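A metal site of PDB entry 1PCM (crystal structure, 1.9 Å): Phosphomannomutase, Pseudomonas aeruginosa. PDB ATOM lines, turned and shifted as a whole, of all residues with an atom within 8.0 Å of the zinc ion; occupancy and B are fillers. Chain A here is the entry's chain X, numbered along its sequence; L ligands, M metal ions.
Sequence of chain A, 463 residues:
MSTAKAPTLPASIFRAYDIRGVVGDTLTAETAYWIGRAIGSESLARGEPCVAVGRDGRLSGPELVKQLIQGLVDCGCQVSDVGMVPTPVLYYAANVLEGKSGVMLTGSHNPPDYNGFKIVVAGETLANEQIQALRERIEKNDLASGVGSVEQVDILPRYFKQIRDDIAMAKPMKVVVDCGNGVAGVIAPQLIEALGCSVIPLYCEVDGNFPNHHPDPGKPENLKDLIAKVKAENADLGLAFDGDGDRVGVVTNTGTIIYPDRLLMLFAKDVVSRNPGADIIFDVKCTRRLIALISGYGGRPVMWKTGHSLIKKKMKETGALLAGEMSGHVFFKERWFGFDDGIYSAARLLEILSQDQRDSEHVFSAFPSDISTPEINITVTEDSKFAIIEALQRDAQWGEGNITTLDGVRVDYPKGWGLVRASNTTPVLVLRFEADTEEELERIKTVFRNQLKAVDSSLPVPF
The side-chain carboxylate of Asp 246 lies within salt-bridge range of the side-chain amino group of Lys 118 (2.8 Å). The backbone carbonyl oxygen (O) of Asp 246 lies within hydrogen-bond range of a ring nitrogen (ND1) of His 329 (3.3 Å). The backbone NH (N) of Asp 242 is in hydrogen-bond range of the backbone carbonyl oxygen (O) of Arg 247. The side-chain carboxylate of Asp 244 lies within salt-bridge range of the side-chain amino group of Lys 118, 3.0 Å away. OD1 of Asp 244 is in hydrogen-bond range of OG1 of Thr 87, at 2.6 Å. NZ of Lys 118 is in salt-bridge range of O2P of SEP 108 (2.7 Å). A ring nitrogen (ND1) of His 109 is in hydrogen-bond range of O1P of SEP 108 (2.5 Å). NH1 of Arg 20 is in salt-bridge range of O2P of SEP 108 (3.2 Å).
The zinc ion is bound by OD1 of Asp 246 (1.9 Å). OD2 of Asp 242 is bound to the zinc ion (1.9 Å). The zinc ion is bound by OD2 of Asp 244 (2.0 Å). O3P of SEP 108 is bound to the zinc ion, at 2.1 Å.
O1 of the ligand is in hydrogen-bond range of O1P of SEP 108, 2.6 Å away. N of His 308 is in hydrogen-bond range of O3 of the ligand, 2.8 Å away. OG of Ser 327 sits at hydrogen-bond distance from O4 of the ligand, 2.7 Å away.
NZ of Lys 118 touches the zinc ion, 3.9 Å away. Five residues have an atom within 4 Å of the zinc ion: SEP 108, Lys 118, Asp 242, Asp 244 and Asp 246.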
ATOM      1  N   ARG A  20      -1.445  11.962  30.861  1.00  0.00           N
ATOM      2  CA  ARG A  20      -0.018  11.836  31.136  1.00  0.00           C
ATOM      3  C   ARG A  20       0.197  10.615  32.001  1.00  0.00           C
ATOM      4  O   ARG A  20      -0.518  10.416  33.000  1.00  0.00           O
ATOM      5  CB  ARG A  20       0.509  13.080  31.839  1.00  0.00           C
ATOM      6  CG  ARG A  20       2.022  13.098  32.129  1.00  0.00           C
ATOM      7  CD  ARG A  20       2.892  13.756  31.053  1.00  0.00           C
ATOM      8  NE  ARG A  20       2.266  14.921  30.432  1.00  0.00           N
ATOM      9  CZ  ARG A  20       2.536  16.197  30.740  1.00  0.00           C
ATOM     10  NH1 ARG A  20       1.896  17.163  30.111  1.00  0.00           N
ATOM     11  NH2 ARG A  20       3.448  16.502  31.655  1.00  0.00           N
ATOM     12  N   ASP A  56       6.502  14.429  20.138  1.00  0.00           N
ATOM     13  CA  ASP A  56       7.735  15.118  20.486  1.00  0.00           C
ATOM     14  C   ASP A  56       8.925  14.184  20.250  1.00  0.00           C
ATOM     15  O   ASP A  56       8.795  13.196  19.514  1.00  0.00           O
ATOM     16  CB  ASP A  56       7.655  15.712  21.886  1.00  0.00           C
ATOM     17  CG  ASP A  56       7.574  14.674  22.986  1.00  0.00           C
ATOM     18  OD1 ASP A  56       7.819  13.464  22.768  1.00  0.00           O
ATOM     19  OD2 ASP A  56       7.290  15.030  24.151  1.00  0.00           O
ATOM     20  N   THR A  87       4.857  20.721  20.112  1.00  0.00           N
ATOM     21  CA  THR A  87       3.436  20.864  20.456  1.00  0.00           C
ATOM     22  C   THR A  87       2.687  21.976  19.713  1.00  0.00           C
ATOM     23  O   THR A  87       1.633  21.712  19.140  1.00  0.00           O
ATOM     24  CB  THR A  87       3.303  21.016  21.979  1.00  0.00           C
ATOM     25  OG1 THR A  87       3.591  19.750  22.593  1.00  0.00           O
ATOM     26  CG2 THR A  87       1.842  21.343  22.384  1.00  0.00           C
ATOM     27  N   PRO A  88       3.173  23.218  19.746  1.00  0.00           N
ATOM     28  CA  PRO A  88       2.476  24.294  19.028  1.00  0.00           C
ATOM     29  C   PRO A  88       2.366  24.067  17.515  1.00  0.00           C
ATOM     30  O   PRO A  88       1.452  24.602  16.890  1.00  0.00           O
ATOM     31  CB  PRO A  88       3.317  25.539  19.344  1.00  0.00           C
ATOM     32  CG  PRO A  88       4.659  24.993  19.753  1.00  0.00           C
ATOM     33  CD  PRO A  88       4.359  23.707  20.464  1.00  0.00           C
ATOM     34  N   TYR A  91      -0.665  22.080  17.154  1.00  0.00           N
ATOM     35  CA  TYR A  91      -1.813  22.983  17.289  1.00  0.00           C
ATOM     36  C   TYR A  91      -2.026  23.800  15.999  1.00  0.00           C
ATOM     37  O   TYR A  91      -3.148  23.984  15.531  1.00  0.00           O
ATOM     38  CB  TYR A  91      -1.637  23.944  18.459  1.00  0.00           C
ATOM     39  CG  TYR A  91      -1.579  23.325  19.853  1.00  0.00           C
ATOM     40  CD1 TYR A  91      -0.920  23.993  20.893  1.00  0.00           C
ATOM     41  CD2 TYR A  91      -2.197  22.108  20.147  1.00  0.00           C
ATOM     42  CE1 TYR A  91      -0.878  23.458  22.183  1.00  0.00           C
ATOM     43  CE2 TYR A  91      -2.155  21.573  21.437  1.00  0.00           C
ATOM     44  CZ  TYR A  91      -1.494  22.246  22.444  1.00  0.00           C
ATOM     45  OH  TYR A  91      -1.433  21.700  23.706  1.00  0.00           O
ATOM     46  N   THR A 106       2.919  13.777  23.801  1.00  0.00           N
ATOM     47  CA  THR A 106       4.009  14.386  24.529  1.00  0.00           C
ATOM     48  C   THR A 106       3.896  14.175  26.037  1.00  0.00           C
ATOM     49  O   THR A 106       2.811  14.022  26.564  1.00  0.00           O
ATOM     50  CB  THR A 106       4.079  15.889  24.197  1.00  0.00           C
ATOM     51  OG1 THR A 106       5.184  16.486  24.887  1.00  0.00           O
ATOM     52  CG2 THR A 106       2.846  16.628  24.714  1.00  0.00           C
ATOM     53  N   GLY A 107       5.051  14.162  26.689  1.00  0.00           N
ATOM     54  CA  GLY A 107       5.158  14.165  28.127  1.00  0.00           C
ATOM     55  C   GLY A 107       5.760  15.449  28.650  1.00  0.00           C
ATOM     56  O   GLY A 107       6.261  15.501  29.774  1.00  0.00           O
ATOM     57  N   SEP A 108       5.734  16.479  27.794  1.00  0.00           N
ATOM     58  CA  SEP A 108       6.012  17.877  28.147  1.00  0.00           C
ATOM     59  CB  SEP A 108       4.878  18.432  29.041  1.00  0.00           C
ATOM     60  OG  SEP A 108       5.160  19.781  29.362  1.00  0.00           O
ATOM     61  C   SEP A 108       7.423  18.108  28.735  1.00  0.00           C
ATOM     62  O   SEP A 108       8.412  17.963  28.021  1.00  0.00           O
ATOM     63  P   SEP A 108       3.973  20.778  29.787  1.00  0.00           P
ATOM     64  O1P SEP A 108       4.247  21.032  31.344  1.00  0.00           O
ATOM     65  O2P SEP A 108       2.484  20.217  29.563  1.00  0.00           O
ATOM     66  O3P SEP A 108       4.152  22.163  29.043  1.00  0.00           O
ATOM     67  N   HIS A 109       7.524  18.453  30.033  1.00  0.00           N
ATOM     68  CA  HIS A 109       8.803  18.763  30.700  1.00  0.00           C
ATOM     69  C   HIS A 109       9.277  17.625  31.624  1.00  0.00           C
ATOM     70  O   HIS A 109      10.327  17.744  32.279  1.00  0.00           O
ATOM     71  CB  HIS A 109       8.709  20.073  31.499  1.00  0.00           C
ATOM     72  CG  HIS A 109       7.678  20.063  32.610  1.00  0.00           C
ATOM     73  ND1 HIS A 109       6.327  19.977  32.369  1.00  0.00           N
ATOM     74  CD2 HIS A 109       7.827  20.175  33.952  1.00  0.00           C
ATOM     75  CE1 HIS A 109       5.672  20.009  33.528  1.00  0.00           C
ATOM     76  NE2 HIS A 109       6.556  20.131  34.503  1.00  0.00           N
ATOM     77  N   ASN A 110       8.493  16.543  31.687  1.00  0.00           N
ATOM     78  CA  ASN A 110       8.717  15.463  32.640  1.00  0.00           C
ATOM     79  C   ASN A 110       9.924  14.577  32.278  1.00  0.00           C
ATOM     80  O   ASN A 110      10.414  14.616  31.147  1.00  0.00           O
ATOM     81  CB  ASN A 110       7.457  14.594  32.759  1.00  0.00           C
ATOM     82  CG  ASN A 110       6.284  15.299  33.447  1.00  0.00           C
ATOM     83  OD1 ASN A 110       5.152  14.922  33.251  1.00  0.00           O
ATOM     84  ND2 ASN A 110       6.572  16.304  34.283  1.00  0.00           N
ATOM     85  N   LYS A 118      -2.023  15.598  24.502  1.00  0.00           N
ATOM     86  CA  LYS A 118      -2.736  16.846  24.576  1.00  0.00           C
ATOM     87  C   LYS A 118      -3.684  16.858  23.373  1.00  0.00           C
ATOM     88  O   LYS A 118      -3.286  16.532  22.238  1.00  0.00           O
ATOM     89  CB  LYS A 118      -1.759  18.021  24.564  1.00  0.00           C
ATOM     90  CG  LYS A 118      -0.831  18.071  25.772  1.00  0.00           C
ATOM     91  CD  LYS A 118       0.228  19.165  25.699  1.00  0.00           C
ATOM     92  CE  LYS A 118       1.061  19.235  26.964  1.00  0.00           C
ATOM     93  NZ  LYS A 118       2.024  20.359  26.938  1.00  0.00           N
ATOM     94  N   PRO A 215      14.480  19.610  30.182  1.00  0.00           N
ATOM     95  CA  PRO A 215      13.982  20.781  29.469  1.00  0.00           C
ATOM     96  C   PRO A 215      12.774  21.410  30.205  1.00  0.00           C
ATOM     97  O   PRO A 215      11.623  21.270  29.793  1.00  0.00           O
ATOM     98  CB  PRO A 215      13.629  20.229  28.083  1.00  0.00           C
ATOM     99  CG  PRO A 215      13.256  18.792  28.324  1.00  0.00           C
ATOM    100  CD  PRO A 215      14.006  18.354  29.576  1.00  0.00           C
ATOM    101  N   PRO A 217      12.382  25.042  31.819  1.00  0.00           N
ATOM    102  CA  PRO A 217      12.881  26.392  32.079  1.00  0.00           C
ATOM    103  C   PRO A 217      12.242  27.110  33.280  1.00  0.00           C
ATOM    104  O   PRO A 217      12.653  28.230  33.583  1.00  0.00           O
ATOM    105  CB  PRO A 217      12.565  27.135  30.778  1.00  0.00           C
ATOM    106  CG  PRO A 217      11.461  26.403  30.179  1.00  0.00           C
ATOM    107  CD  PRO A 217      11.606  24.978  30.576  1.00  0.00           C
ATOM    108  N   PHE A 241      13.741  26.655  26.032  1.00  0.00           N
ATOM    109  CA  PHE A 241      12.454  26.032  25.712  1.00  0.00           C
ATOM    110  C   PHE A 241      12.253  24.788  26.555  1.00  0.00           C
ATOM    111  O   PHE A 241      13.222  24.138  26.928  1.00  0.00           O
ATOM    112  CB  PHE A 241      12.385  25.709  24.230  1.00  0.00           C
ATOM    113  CG  PHE A 241      12.429  26.927  23.362  1.00  0.00           C
ATOM    114  CD1 PHE A 241      11.305  27.721  23.214  1.00  0.00           C
ATOM    115  CD2 PHE A 241      13.597  27.306  22.752  1.00  0.00           C
ATOM    116  CE1 PHE A 241      11.352  28.858  22.444  1.00  0.00           C
ATOM    117  CE2 PHE A 241      13.639  28.465  21.973  1.00  0.00           C
ATOM    118  CZ  PHE A 241      12.517  29.237  21.825  1.00  0.00           C
ATOM    119  N   ASP A 242      11.007  24.473  26.882  1.00  0.00           N
ATOM    120  CA  ASP A 242      10.712  23.210  27.548  1.00  0.00           C
ATOM    121  C   ASP A 242      10.686  22.094  26.520  1.00  0.00           C
ATOM    122  O   ASP A 242      10.886  22.327  25.320  1.00  0.00           O
ATOM    123  CB  ASP A 242       9.443  23.291  28.404  1.00  0.00           C
ATOM    124  CG  ASP A 242       8.154  23.061  27.620  1.00  0.00           C
ATOM    125  OD1 ASP A 242       8.079  23.372  26.394  1.00  0.00           O
ATOM    126  OD2 ASP A 242       7.162  22.594  28.188  1.00  0.00           O
ATOM    127  N   GLY A 243      10.460  20.866  26.965  1.00  0.00           N
ATOM    128  CA  GLY A 243      10.651  19.716  26.101  1.00  0.00           C
ATOM    129  C   GLY A 243       9.855  19.704  24.810  1.00  0.00           C
ATOM    130  O   GLY A 243      10.359  19.223  23.790  1.00  0.00           O
ATOM    131  N   ASP A 244       8.621  20.210  24.833  1.00  0.00           N
ATOM    132  CA  ASP A 244       7.740  20.161  23.660  1.00  0.00           C
ATOM    133  C   ASP A 244       7.507  21.519  23.000  1.00  0.00           C
ATOM    134  O   ASP A 244       6.768  21.616  22.025  1.00  0.00           O
ATOM    135  CB  ASP A 244       6.405  19.495  24.003  1.00  0.00           C
ATOM    136  CG  ASP A 244       5.605  20.253  25.061  1.00  0.00           C
ATOM    137  OD1 ASP A 244       4.361  20.219  25.023  1.00  0.00           O
ATOM    138  OD2 ASP A 244       6.148  20.878  25.986  1.00  0.00           O
ATOM    139  N   GLY A 245       8.149  22.556  23.528  1.00  0.00           N
ATOM    140  CA  GLY A 245       8.179  23.862  22.898  1.00  0.00           C
ATOM    141  C   GLY A 245       6.999  24.797  23.098  1.00  0.00           C
ATOM    142  O   GLY A 245       6.896  25.813  22.390  1.00  0.00           O
ATOM    143  N   ASP A 246       6.112  24.497  24.048  1.00  0.00           N
ATOM    144  CA  ASP A 246       4.980  25.392  24.359  1.00  0.00           C
ATOM    145  C   ASP A 246       5.254  26.359  25.513  1.00  0.00           C
ATOM    146  O   ASP A 246       4.419  27.202  25.852  1.00  0.00           O
ATOM    147  CB  ASP A 246       3.677  24.608  24.577  1.00  0.00           C
ATOM    148  CG  ASP A 246       3.763  23.588  25.676  1.00  0.00           C
ATOM    149  OD1 ASP A 246       4.785  23.479  26.383  1.00  0.00           O
ATOM    150  OD2 ASP A 246       2.806  22.820  25.922  1.00  0.00           O
ATOM    151  N   ARG A 247       6.454  26.243  26.088  1.00  0.00           N
ATOM    152  CA  ARG A 247       6.902  27.126  27.156  1.00  0.00           C
ATOM    153  C   ARG A 247       8.247  27.722  26.791  1.00  0.00           C
ATOM    154  O   ARG A 247       9.093  27.057  26.194  1.00  0.00           O
ATOM    155  CB  ARG A 247       7.007  26.351  28.475  1.00  0.00           C
ATOM    156  N   VAL A 248       8.436  28.984  27.173  1.00  0.00           N
ATOM    157  CA  VAL A 248       9.705  29.669  26.940  1.00  0.00           C
ATOM    158  C   VAL A 248      10.121  30.359  28.254  1.00  0.00           C
ATOM    159  O   VAL A 248       9.271  30.771  29.055  1.00  0.00           O
ATOM    160  CB  VAL A 248       9.597  30.674  25.764  1.00  0.00           C
ATOM    161  CG1 VAL A 248       8.547  31.771  26.047  1.00  0.00           C
ATOM    162  CG2 VAL A 248      10.932  31.282  25.455  1.00  0.00           C
ATOM    163  N   HIS A 308      -3.039  25.046  30.829  1.00  0.00           N
ATOM    164  CA  HIS A 308      -3.091  25.467  29.418  1.00  0.00           C
ATOM    165  C   HIS A 308      -4.449  25.314  28.765  1.00  0.00           C
ATOM    166  O   HIS A 308      -4.938  26.234  28.101  1.00  0.00           O
ATOM    167  CB  HIS A 308      -2.014  24.761  28.596  1.00  0.00           C
ATOM    168  CG  HIS A 308      -2.246  23.287  28.389  1.00  0.00           C
ATOM    169  ND1 HIS A 308      -2.208  22.701  27.144  1.00  0.00           N
ATOM    170  CD2 HIS A 308      -2.572  22.304  29.258  1.00  0.00           C
ATOM    171  CE1 HIS A 308      -2.433  21.407  27.259  1.00  0.00           C
ATOM    172  NE2 HIS A 308      -2.666  21.143  28.526  1.00  0.00           N
ATOM    173  N   SER A 327       3.732  29.717  34.467  1.00  0.00           N
ATOM    174  CA  SER A 327       4.549  28.576  34.028  1.00  0.00           C
ATOM    175  C   SER A 327       5.277  28.823  32.702  1.00  0.00           C
ATOM    176  O   SER A 327       6.073  28.004  32.291  1.00  0.00           O
ATOM    177  CB  SER A 327       3.683  27.320  33.905  1.00  0.00           C
ATOM    178  OG  SER A 327       2.640  27.536  32.966  1.00  0.00           O
ATOM    179  N   HIS A 329       3.686  29.457  29.653  1.00  0.00           N
ATOM    180  CA  HIS A 329       2.823  29.253  28.480  1.00  0.00           C
ATOM    181  C   HIS A 329       2.282  30.611  28.098  1.00  0.00           C
ATOM    182  O   HIS A 329       1.654  31.273  28.922  1.00  0.00           O
ATOM    183  CB  HIS A 329       1.663  28.259  28.758  1.00  0.00           C
ATOM    184  CG  HIS A 329       2.135  26.871  29.018  1.00  0.00           C
ATOM    185  ND1 HIS A 329       2.300  25.943  28.027  1.00  0.00           N
ATOM    186  CD2 HIS A 329       2.512  26.252  30.163  1.00  0.00           C
ATOM    187  CE1 HIS A 329       2.779  24.820  28.542  1.00  0.00           C
ATOM    188  NE2 HIS A 329       2.924  24.990  29.840  1.00  0.00           N
ATOM    189  N   ASP A 340      -0.911  28.240  22.961  1.00  0.00           N
ATOM    190  CA  ASP A 340       0.373  28.439  23.610  1.00  0.00           C
ATOM    191  C   ASP A 340       1.528  27.912  22.740  1.00  0.00           C
ATOM    192  O   ASP A 340       1.439  26.833  22.184  1.00  0.00           O
ATOM    193  CB  ASP A 340       0.426  27.833  25.006  1.00  0.00           C
ATOM    194  CG  ASP A 340      -0.186  26.433  25.112  1.00  0.00           C
ATOM    195  OD1 ASP A 340       0.264  25.674  26.020  1.00  0.00           O
ATOM    196  OD2 ASP A 340      -1.152  26.022  24.415  1.00  0.00           O
HETATM  197  C1  LIG L   1       1.917  22.330  33.103  1.00  0.00           C
HETATM  198  C2  LIG L   1       0.943  22.954  32.122  1.00  0.00           C
HETATM  199  C3  LIG L   1       0.730  24.459  32.444  1.00  0.00           C
HETATM  200  C4  LIG L   1       0.518  24.751  33.939  1.00  0.00           C
HETATM  201  C5  LIG L   1       1.536  23.974  34.801  1.00  0.00           C
HETATM  202  C6  LIG L   1       1.171  24.163  36.272  1.00  0.00           C
HETATM  203  O1  LIG L   1       3.220  22.867  32.874  1.00  0.00           O
HETATM  204  O2  LIG L   1      -0.333  22.263  32.186  1.00  0.00           O
HETATM  205  O3  LIG L   1      -0.419  24.901  31.741  1.00  0.00           O
HETATM  206  O4  LIG L   1       0.665  26.139  34.160  1.00  0.00           O
HETATM  207  O5  LIG L   1       1.489  22.589  34.477  1.00  0.00           O
HETATM  208  O6  LIG L   1       0.046  23.259  36.577  1.00  0.00           O
HETATM  209  P1  LIG L   1      -0.389  23.013  38.112  1.00  0.00           P
HETATM  210  O7  LIG L   1      -0.117  24.282  38.837  1.00  0.00           O
HETATM  211  O8  LIG L   1       0.416  21.885  38.685  1.00  0.00           O
HETATM  212  O9  LIG L   1      -1.836  22.627  38.123  1.00  0.00           O
HETATM  213 ZN    ZN M   1       5.459  22.047  27.424  1.00  0.00          ZN
